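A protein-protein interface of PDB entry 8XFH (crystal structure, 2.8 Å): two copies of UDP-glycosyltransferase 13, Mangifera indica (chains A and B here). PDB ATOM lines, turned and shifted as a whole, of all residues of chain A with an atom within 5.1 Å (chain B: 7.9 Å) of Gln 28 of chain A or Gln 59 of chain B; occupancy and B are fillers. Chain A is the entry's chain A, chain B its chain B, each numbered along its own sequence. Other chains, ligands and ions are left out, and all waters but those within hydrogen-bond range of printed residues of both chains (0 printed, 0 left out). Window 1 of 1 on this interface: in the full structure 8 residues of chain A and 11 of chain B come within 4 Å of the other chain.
NE2 of His 30 of chain A lies within hydrogen-bond range of O of Gln 59 of chain B (3.4 Å).
Among the printed residues, pairs that only touch across the chains: His 30 of chain A with Arg 32 of chain B (3.4 Å), Gln 59 of chain A with Gln 28 of chain B (3.6 Å), Gln 28 of chain A with Gln 59 of chain B (3.7 Å), Gln 28 of chain A with Pro 58 of chain B (3.8 Å) and Gln 59 of chain A with Val 27 of chain B (3.8 Å).
Of the printed residues of chain A, Gln 59 of chain B touches Gln 28 (3.7 Å) and His 30 (3.4 Å).
Of the printed residues of chain B, Gln 59 of chain A touches Val 27 (3.8 Å) and Gln 28 (3.6 Å).
Of the printed residues of chain A, Arg 32 of chain B touches His 30.
Leu 54 of chain B touches none of the printed residues of chain A.
The nearest residue of chain A that does not touch Gln 59 of chain B is Gln 59 of chain A (4.1 Å).
Of the 18 printed residues of chain B, 5 touch a printed residue of chain A.
Hydrophobic or aromatic side chains of chain B within 4 Å of the printed part of chain A: Pro 58.
Along chain B the printed residues that touch a printed residue of chain A span positions 27 to 59.
Of the 9 printed residues of chain A, 3 touch a printed residue of chain B.
Printed residues of chain A that touch a printed residue of chain B: Gln 28, His 30 and Gln 59.
Hydrophobic or aromatic side chains of chain A within 4 Å of the printed part of chain B: His 30.
Among the printed residues, 6 pairs touch across the chains.
Among the printed residues, no Asp or Glu carboxylate lies within 4 Å of a Lys or Arg side-chain nitrogen of the other chain.
Gln 28 of chain A touches Gln 59 of chain B, and with the chains exchanged Gln 59 of chain A touches Gln 28 of chain B.
Gln 59 of chain A touches Val 27 of chain B, but with the chains exchanged Val 27 of chain A does not touch Gln 59 of chain B (4.2 Å).
5 positions are printed for both chains.
Of the 6 pairs that touch across the chains among the printed residues, 2 have their exchanged pair printed and touching as well.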
ATOM      1  N   ALA A  24      -1.550   8.497 -15.332  1.00  0.00           N
ATOM      2  CA  ALA A  24      -1.609   8.876 -16.735  1.00  0.00           C
ATOM      3  C   ALA A  24      -0.639   8.038 -17.565  1.00  0.00           C
ATOM      4  O   ALA A  24      -0.976   7.577 -18.658  1.00  0.00           O
ATOM      5  CB  ALA A  24      -1.304  10.359 -16.896  1.00  0.00           C
ATOM      6  N   THR A  25       0.566   7.845 -17.038  1.00  0.00           N
ATOM      7  CA  THR A  25       1.578   7.044 -17.715  1.00  0.00           C
ATOM      8  C   THR A  25       1.083   5.610 -17.913  1.00  0.00           C
ATOM      9  O   THR A  25       1.265   5.021 -18.980  1.00  0.00           O
ATOM     10  CB  THR A  25       2.905   7.036 -16.931  1.00  0.00           C
ATOM     11  OG1 THR A  25       3.348   8.384 -16.725  1.00  0.00           O
ATOM     12  CG2 THR A  25       3.978   6.267 -17.690  1.00  0.00           C
ATOM     13  N   LEU A  26       0.439   5.065 -16.884  1.00  0.00           N
ATOM     14  CA  LEU A  26      -0.129   3.719 -16.944  1.00  0.00           C
ATOM     15  C   LEU A  26      -1.203   3.591 -18.027  1.00  0.00           C
ATOM     16  O   LEU A  26      -1.159   2.677 -18.854  1.00  0.00           O
ATOM     17  CB  LEU A  26      -0.719   3.329 -15.587  1.00  0.00           C
ATOM     18  CG  LEU A  26       0.216   2.749 -14.526  1.00  0.00           C
ATOM     19  CD1 LEU A  26      -0.548   2.507 -13.240  1.00  0.00           C
ATOM     20  CD2 LEU A  26       0.836   1.460 -15.029  1.00  0.00           C
ATOM     21  N   VAL A  27      -2.167   4.507 -18.003  1.00  0.00           N
ATOM     22  CA  VAL A  27      -3.268   4.525 -18.965  1.00  0.00           C
ATOM     23  C   VAL A  27      -2.757   4.622 -20.406  1.00  0.00           C
ATOM     24  O   VAL A  27      -3.334   4.032 -21.327  1.00  0.00           O
ATOM     25  CB  VAL A  27      -4.246   5.697 -18.661  1.00  0.00           C
ATOM     26  CG1 VAL A  27      -4.663   6.435 -19.932  1.00  0.00           C
ATOM     27  CG2 VAL A  27      -5.465   5.193 -17.899  1.00  0.00           C
ATOM     28  N   GLN A  28      -1.657   5.343 -20.590  1.00  0.00           N
ATOM     29  CA  GLN A  28      -1.058   5.501 -21.909  1.00  0.00           C
ATOM     30  C   GLN A  28      -0.217   4.285 -22.274  1.00  0.00           C
ATOM     31  O   GLN A  28       0.311   4.194 -23.382  1.00  0.00           O
ATOM     32  CB  GLN A  28      -0.208   6.772 -21.960  1.00  0.00           C
ATOM     33  CG  GLN A  28      -1.016   8.056 -21.837  1.00  0.00           C
ATOM     34  CD  GLN A  28      -0.144   9.295 -21.767  1.00  0.00           C
ATOM     35  OE1 GLN A  28       1.082   9.202 -21.752  1.00  0.00           O
ATOM     36  NE2 GLN A  28      -0.774  10.464 -21.724  1.00  0.00           N
ATOM     37  N   HIS A  29      -0.090   3.356 -21.332  1.00  0.00           N
ATOM     38  CA  HIS A  29       0.643   2.120 -21.572  1.00  0.00           C
ATOM     39  C   HIS A  29      -0.289   0.915 -21.504  1.00  0.00           C
ATOM     40  O   HIS A  29       0.104  -0.165 -21.057  1.00  0.00           O
ATOM     41  CB  HIS A  29       1.787   1.970 -20.573  1.00  0.00           C
ATOM     42  CG  HIS A  29       2.949   2.873 -20.844  1.00  0.00           C
ATOM     43  ND1 HIS A  29       2.950   4.208 -20.507  1.00  0.00           N
ATOM     44  CD2 HIS A  29       4.151   2.629 -21.420  1.00  0.00           C
ATOM     45  CE1 HIS A  29       4.101   4.750 -20.863  1.00  0.00           C
ATOM     46  NE2 HIS A  29       4.847   3.812 -21.420  1.00  0.00           N
ATOM     47  N   HIS A  30      -1.528   1.125 -21.945  1.00  0.00           N
ATOM     48  CA  HIS A  30      -2.539   0.075 -22.058  1.00  0.00           C
ATOM     49  C   HIS A  30      -2.849  -0.614 -20.729  1.00  0.00           C
ATOM     50  O   HIS A  30      -2.876  -1.844 -20.645  1.00  0.00           O
ATOM     51  CB  HIS A  30      -2.105  -0.958 -23.098  1.00  0.00           C
ATOM     52  CG  HIS A  30      -1.747  -0.359 -24.423  1.00  0.00           C
ATOM     53  ND1 HIS A  30      -0.443  -0.174 -24.827  1.00  0.00           N
ATOM     54  CD2 HIS A  30      -2.523   0.111 -25.429  1.00  0.00           C
ATOM     55  CE1 HIS A  30      -0.430   0.375 -26.029  1.00  0.00           C
ATOM     56  NE2 HIS A  30      -1.679   0.558 -26.417  1.00  0.00           N
ATOM     57  N   PHE A  57      -8.904  12.634 -18.672  1.00  0.00           N
ATOM     58  CA  PHE A  57      -8.865  11.178 -18.781  1.00  0.00           C
ATOM     59  C   PHE A  57     -10.158  10.558 -18.253  1.00  0.00           C
ATOM     60  O   PHE A  57     -10.199  10.065 -17.124  1.00  0.00           O
ATOM     61  CB  PHE A  57      -7.654  10.604 -18.033  1.00  0.00           C
ATOM     62  CG  PHE A  57      -6.325  11.021 -18.606  1.00  0.00           C
ATOM     63  CD1 PHE A  57      -5.747  10.308 -19.645  1.00  0.00           C
ATOM     64  CD2 PHE A  57      -5.649  12.122 -18.101  1.00  0.00           C
ATOM     65  CE1 PHE A  57      -4.522  10.687 -20.175  1.00  0.00           C
ATOM     66  CE2 PHE A  57      -4.424  12.504 -18.630  1.00  0.00           C
ATOM     67  CZ  PHE A  57      -3.863  11.785 -19.665  1.00  0.00           C
ATOM     68  N   GLN A  59     -11.454   7.837 -18.981  1.00  0.00           N
ATOM     69  CA  GLN A  59     -11.316   6.396 -18.802  1.00  0.00           C
ATOM     70  C   GLN A  59     -10.720   6.041 -17.439  1.00  0.00           C
ATOM     71  O   GLN A  59     -10.622   4.867 -17.081  1.00  0.00           O
ATOM     72  CB  GLN A  59     -10.458   5.800 -19.922  1.00  0.00           C
ATOM     73  CG  GLN A  59      -9.016   6.308 -19.969  1.00  0.00           C
ATOM     74  CD  GLN A  59      -8.871   7.618 -20.724  1.00  0.00           C
ATOM     75  OE1 GLN A  59      -9.745   8.479 -20.664  1.00  0.00           O
ATOM     76  NE2 GLN A  59      -7.767   7.768 -21.447  1.00  0.00           N
ATOM     77  N   HIS B   4      -9.521  -4.281 -29.635  1.00  0.00           N
ATOM     78  CA  HIS B   4      -8.714  -3.480 -30.548  1.00  0.00           C
ATOM     79  C   HIS B   4      -9.519  -3.090 -31.785  1.00  0.00           C
ATOM     80  O   HIS B   4      -9.931  -3.953 -32.562  1.00  0.00           O
ATOM     81  CB  HIS B   4      -7.449  -4.245 -30.952  1.00  0.00           C
ATOM     82  CG  HIS B   4      -6.371  -3.374 -31.517  1.00  0.00           C
ATOM     83  ND1 HIS B   4      -5.092  -3.832 -31.757  1.00  0.00           N
ATOM     84  CD2 HIS B   4      -6.378  -2.071 -31.886  1.00  0.00           C
ATOM     85  CE1 HIS B   4      -4.359  -2.850 -32.250  1.00  0.00           C
ATOM     86  NE2 HIS B   4      -5.117  -1.769 -32.339  1.00  0.00           N
ATOM     87  N   ALA B  24     -11.018   8.831 -30.122  1.00  0.00           N
ATOM     88  CA  ALA B  24     -10.814   9.226 -28.735  1.00  0.00           C
ATOM     89  C   ALA B  24     -11.922   8.674 -27.839  1.00  0.00           C
ATOM     90  O   ALA B  24     -11.659   8.239 -26.718  1.00  0.00           O
ATOM     91  CB  ALA B  24     -10.739  10.741 -28.621  1.00  0.00           C
ATOM     92  N   VAL B  27     -11.171   5.075 -26.947  1.00  0.00           N
ATOM     93  CA  VAL B  27     -10.123   4.973 -25.934  1.00  0.00           C
ATOM     94  C   VAL B  27     -10.671   5.300 -24.549  1.00  0.00           C
ATOM     95  O   VAL B  27     -10.341   4.640 -23.562  1.00  0.00           O
ATOM     96  CB  VAL B  27      -8.941   5.913 -26.244  1.00  0.00           C
ATOM     97  CG1 VAL B  27      -7.824   5.726 -25.230  1.00  0.00           C
ATOM     98  CG2 VAL B  27      -8.425   5.663 -27.645  1.00  0.00           C
ATOM     99  N   GLN B  28     -11.529   6.313 -24.485  1.00  0.00           N
ATOM    100  CA  GLN B  28     -12.149   6.721 -23.230  1.00  0.00           C
ATOM    101  C   GLN B  28     -13.185   5.698 -22.763  1.00  0.00           C
ATOM    102  O   GLN B  28     -13.659   5.758 -21.628  1.00  0.00           O
ATOM    103  CB  GLN B  28     -12.789   8.108 -23.379  1.00  0.00           C
ATOM    104  CG  GLN B  28     -11.788   9.222 -23.688  1.00  0.00           C
ATOM    105  CD  GLN B  28     -12.455  10.503 -24.170  1.00  0.00           C
ATOM    106  OE1 GLN B  28     -13.678  10.626 -24.141  1.00  0.00           O
ATOM    107  NE2 GLN B  28     -11.649  11.460 -24.621  1.00  0.00           N
ATOM    108  N   CYS B  31     -10.893   0.938 -25.131  1.00  0.00           N
ATOM    109  CA  CYS B  31     -10.522   0.199 -26.336  1.00  0.00           C
ATOM    110  C   CYS B  31      -9.141   0.632 -26.808  1.00  0.00           C
ATOM    111  O   CYS B  31      -8.765   1.796 -26.648  1.00  0.00           O
ATOM    112  CB  CYS B  31     -11.541   0.422 -27.456  1.00  0.00           C
ATOM    113  SG  CYS B  31     -13.194  -0.219 -27.141  1.00  0.00           S
ATOM    114  N   ARG B  32      -8.388  -0.300 -27.383  1.00  0.00           N
ATOM    115  CA  ARG B  32      -7.145   0.055 -28.050  1.00  0.00           C
ATOM    116  C   ARG B  32      -7.474   0.466 -29.476  1.00  0.00           C
ATOM    117  O   ARG B  32      -8.192  -0.244 -30.180  1.00  0.00           O
ATOM    118  CB  ARG B  32      -6.153  -1.105 -28.037  1.00  0.00           C
ATOM    119  CG  ARG B  32      -4.776  -0.741 -28.584  1.00  0.00           C
ATOM    120  CD  ARG B  32      -3.829  -1.928 -28.547  1.00  0.00           C
ATOM    121  NE  ARG B  32      -3.789  -2.542 -27.224  1.00  0.00           N
ATOM    122  CZ  ARG B  32      -2.699  -3.065 -26.673  1.00  0.00           C
ATOM    123  NH1 ARG B  32      -2.759  -3.600 -25.461  1.00  0.00           N
ATOM    124  NH2 ARG B  32      -1.546  -3.051 -27.329  1.00  0.00           N
ATOM    125  N   VAL B  33      -6.958   1.611 -29.903  1.00  0.00           N
ATOM    126  CA  VAL B  33      -7.333   2.149 -31.202  1.00  0.00           C
ATOM    127  C   VAL B  33      -6.133   2.274 -32.132  1.00  0.00           C
ATOM    128  O   VAL B  33      -5.100   2.834 -31.762  1.00  0.00           O
ATOM    129  CB  VAL B  33      -8.019   3.523 -31.048  1.00  0.00           C
ATOM    130  CG1 VAL B  33      -8.253   4.167 -32.406  1.00  0.00           C
ATOM    131  CG2 VAL B  33      -9.331   3.374 -30.291  1.00  0.00           C
ATOM    132  N   THR B  34      -6.273   1.724 -33.334  1.00  0.00           N
ATOM    133  CA  THR B  34      -5.283   1.907 -34.385  1.00  0.00           C
ATOM    134  C   THR B  34      -5.935   2.612 -35.566  1.00  0.00           C
ATOM    135  O   THR B  34      -6.880   2.091 -36.156  1.00  0.00           O
ATOM    136  CB  THR B  34      -4.685   0.574 -34.859  1.00  0.00           C
ATOM    137  OG1 THR B  34      -4.062  -0.095 -33.758  1.00  0.00           O
ATOM    138  CG2 THR B  34      -3.653   0.816 -35.953  1.00  0.00           C
ATOM    139  N   LEU B  53      -3.760  14.507 -32.368  1.00  0.00           N
ATOM    140  CA  LEU B  53      -4.425  13.365 -31.748  1.00  0.00           C
ATOM    141  C   LEU B  53      -3.394  12.336 -31.299  1.00  0.00           C
ATOM    142  O   LEU B  53      -3.483  11.790 -30.198  1.00  0.00           O
ATOM    143  CB  LEU B  53      -5.423  12.717 -32.709  1.00  0.00           C
ATOM    144  CG  LEU B  53      -6.230  11.580 -32.078  1.00  0.00           C
ATOM    145  CD1 LEU B  53      -7.439  12.136 -31.341  1.00  0.00           C
ATOM    146  CD2 LEU B  53      -6.639  10.543 -33.111  1.00  0.00           C
ATOM    147  N   LEU B  54      -2.417  12.072 -32.162  1.00  0.00           N
ATOM    148  CA  LEU B  54      -1.344  11.137 -31.844  1.00  0.00           C
ATOM    149  C   LEU B  54      -0.476  11.667 -30.704  1.00  0.00           C
ATOM    150  O   LEU B  54       0.095  10.892 -29.934  1.00  0.00           O
ATOM    151  CB  LEU B  54      -0.480  10.859 -33.077  1.00  0.00           C
ATOM    152  CG  LEU B  54      -1.100  10.030 -34.201  1.00  0.00           C
ATOM    153  CD1 LEU B  54      -0.057   9.709 -35.256  1.00  0.00           C
ATOM    154  CD2 LEU B  54      -1.723   8.755 -33.651  1.00  0.00           C
ATOM    155  N   SER B  55      -0.383  12.989 -30.598  1.00  0.00           N
ATOM    156  CA  SER B  55       0.425  13.622 -29.559  1.00  0.00           C
ATOM    157  C   SER B  55      -0.258  13.563 -28.197  1.00  0.00           C
ATOM    158  O   SER B  55       0.406  13.490 -27.162  1.00  0.00           O
ATOM    159  CB  SER B  55       0.723  15.077 -29.928  1.00  0.00           C
ATOM    160  OG  SER B  55       1.478  15.712 -28.913  1.00  0.00           O
ATOM    161  N   ASP B  56      -1.585  13.596 -28.206  1.00  0.00           N
ATOM    162  CA  ASP B  56      -2.367  13.594 -26.976  1.00  0.00           C
ATOM    163  C   ASP B  56      -2.846  12.190 -26.609  1.00  0.00           C
ATOM    164  O   ASP B  56      -3.261  11.950 -25.477  1.00  0.00           O
ATOM    165  CB  ASP B  56      -3.559  14.548 -27.104  1.00  0.00           C
ATOM    166  CG  ASP B  56      -3.182  15.993 -26.828  1.00  0.00           C
ATOM    167  OD1 ASP B  56      -2.679  16.671 -27.750  1.00  0.00           O
ATOM    168  OD2 ASP B  56      -3.394  16.449 -25.685  1.00  0.00           O
ATOM    169  N   PHE B  57      -2.786  11.268 -27.565  1.00  0.00           N
ATOM    170  CA  PHE B  57      -3.136   9.872 -27.305  1.00  0.00           C
ATOM    171  C   PHE B  57      -2.029   8.922 -27.762  1.00  0.00           C
ATOM    172  O   PHE B  57      -2.135   8.305 -28.824  1.00  0.00           O
ATOM    173  CB  PHE B  57      -4.453   9.504 -27.993  1.00  0.00           C
ATOM    174  CG  PHE B  57      -5.671  10.102 -27.346  1.00  0.00           C
ATOM    175  CD1 PHE B  57      -6.127  11.359 -27.718  1.00  0.00           C
ATOM    176  CD2 PHE B  57      -6.371   9.401 -26.377  1.00  0.00           C
ATOM    177  CE1 PHE B  57      -7.255  11.909 -27.126  1.00  0.00           C
ATOM    178  CE2 PHE B  57      -7.497   9.947 -25.784  1.00  0.00           C
ATOM    179  CZ  PHE B  57      -7.938  11.202 -26.159  1.00  0.00           C
ATOM    180  N   PRO B  58      -0.962   8.800 -26.954  1.00  0.00           N
ATOM    181  CA  PRO B  58       0.181   7.929 -27.256  1.00  0.00           C
ATOM    182  C   PRO B  58      -0.198   6.455 -27.390  1.00  0.00           C
ATOM    183  O   PRO B  58       0.492   5.706 -28.086  1.00  0.00           O
ATOM    184  CB  PRO B  58       1.108   8.140 -26.053  1.00  0.00           C
ATOM    185  CG  PRO B  58       0.737   9.477 -25.519  1.00  0.00           C
ATOM    186  CD  PRO B  58      -0.742   9.583 -25.726  1.00  0.00           C
ATOM    187  N   GLN B  59      -1.282   6.049 -26.736  1.00  0.00           N
ATOM    188  CA  GLN B  59      -1.726   4.660 -26.783  1.00  0.00           C
ATOM    189  C   GLN B  59      -2.389   4.327 -28.118  1.00  0.00           C
ATOM    190  O   GLN B  59      -2.487   3.158 -28.490  1.00  0.00           O
ATOM    191  CB  GLN B  59      -2.684   4.359 -25.625  1.00  0.00           C
ATOM    192  CG  GLN B  59      -3.952   5.200 -25.591  1.00  0.00           C
ATOM    193  CD  GLN B  59      -3.755   6.540 -24.913  1.00  0.00           C
ATOM    194  OE1 GLN B  59      -2.730   7.195 -25.090  1.00  0.00           O
ATOM    195  NE2 GLN B  59      -4.741   6.954 -24.126  1.00  0.00           N
ATOM    196  N   ILE B  60      -2.850   5.352 -28.831  1.00  0.00           N
ATOM    197  CA  ILE B  60      -3.383   5.162 -30.176  1.00  0.00           C
ATOM    198  C   ILE B  60      -2.229   5.007 -31.156  1.00  0.00           C
ATOM    199  O   ILE B  60      -1.292   5.809 -31.151  1.00  0.00           O
ATOM    200  CB  ILE B  60      -4.281   6.336 -30.617  1.00  0.00           C
ATOM    201  CG1 ILE B  60      -5.511   6.446 -29.716  1.00  0.00           C
ATOM    202  CG2 ILE B  60      -4.714   6.172 -32.066  1.00  0.00           C
ATOM    203  CD1 ILE B  60      -6.512   7.482 -30.179  1.00  0.00           C
ATOM    204  N   THR B  61      -2.299   3.975 -31.993  1.00  0.00           N
ATOM    205  CA  THR B  61      -1.224   3.671 -32.929  1.00  0.00           C
ATOM    206  C   THR B  61      -1.617   4.041 -34.363  1.00  0.00           C
ATOM    207  O   THR B  61      -2.757   3.827 -34.777  1.00  0.00           O
ATOM    208  CB  THR B  61      -0.841   2.182 -32.859  1.00  0.00           C
ATOM    209  OG1 THR B  61      -0.556   1.825 -31.500  1.00  0.00           O
ATOM    210  CG2 THR B  61       0.383   1.893 -33.719  1.00  0.00           C
ATOM    211  N   GLU B  62      -0.671   4.609 -35.108  1.00  0.00           N
ATOM    212  CA  GLU B  62      -0.904   4.999 -36.496  1.00  0.00           C
ATOM    213  C   GLU B  62      -0.161   4.084 -37.469  1.00  0.00           C
ATOM    214  O   GLU B  62       1.064   3.965 -37.406  1.00  0.00           O
ATOM    215  CB  GLU B  62      -0.474   6.450 -36.721  1.00  0.00           C
ATOM    216  CG  GLU B  62      -0.505   6.901 -38.178  1.00  0.00           C
ATOM    217  CD  GLU B  62       0.391   8.099 -38.437  1.00  0.00           C
ATOM    218  OE1 GLU B  62       1.446   8.211 -37.776  1.00  0.00           O
ATOM    219  OE2 GLU B  62       0.042   8.930 -39.299  1.00  0.00           O
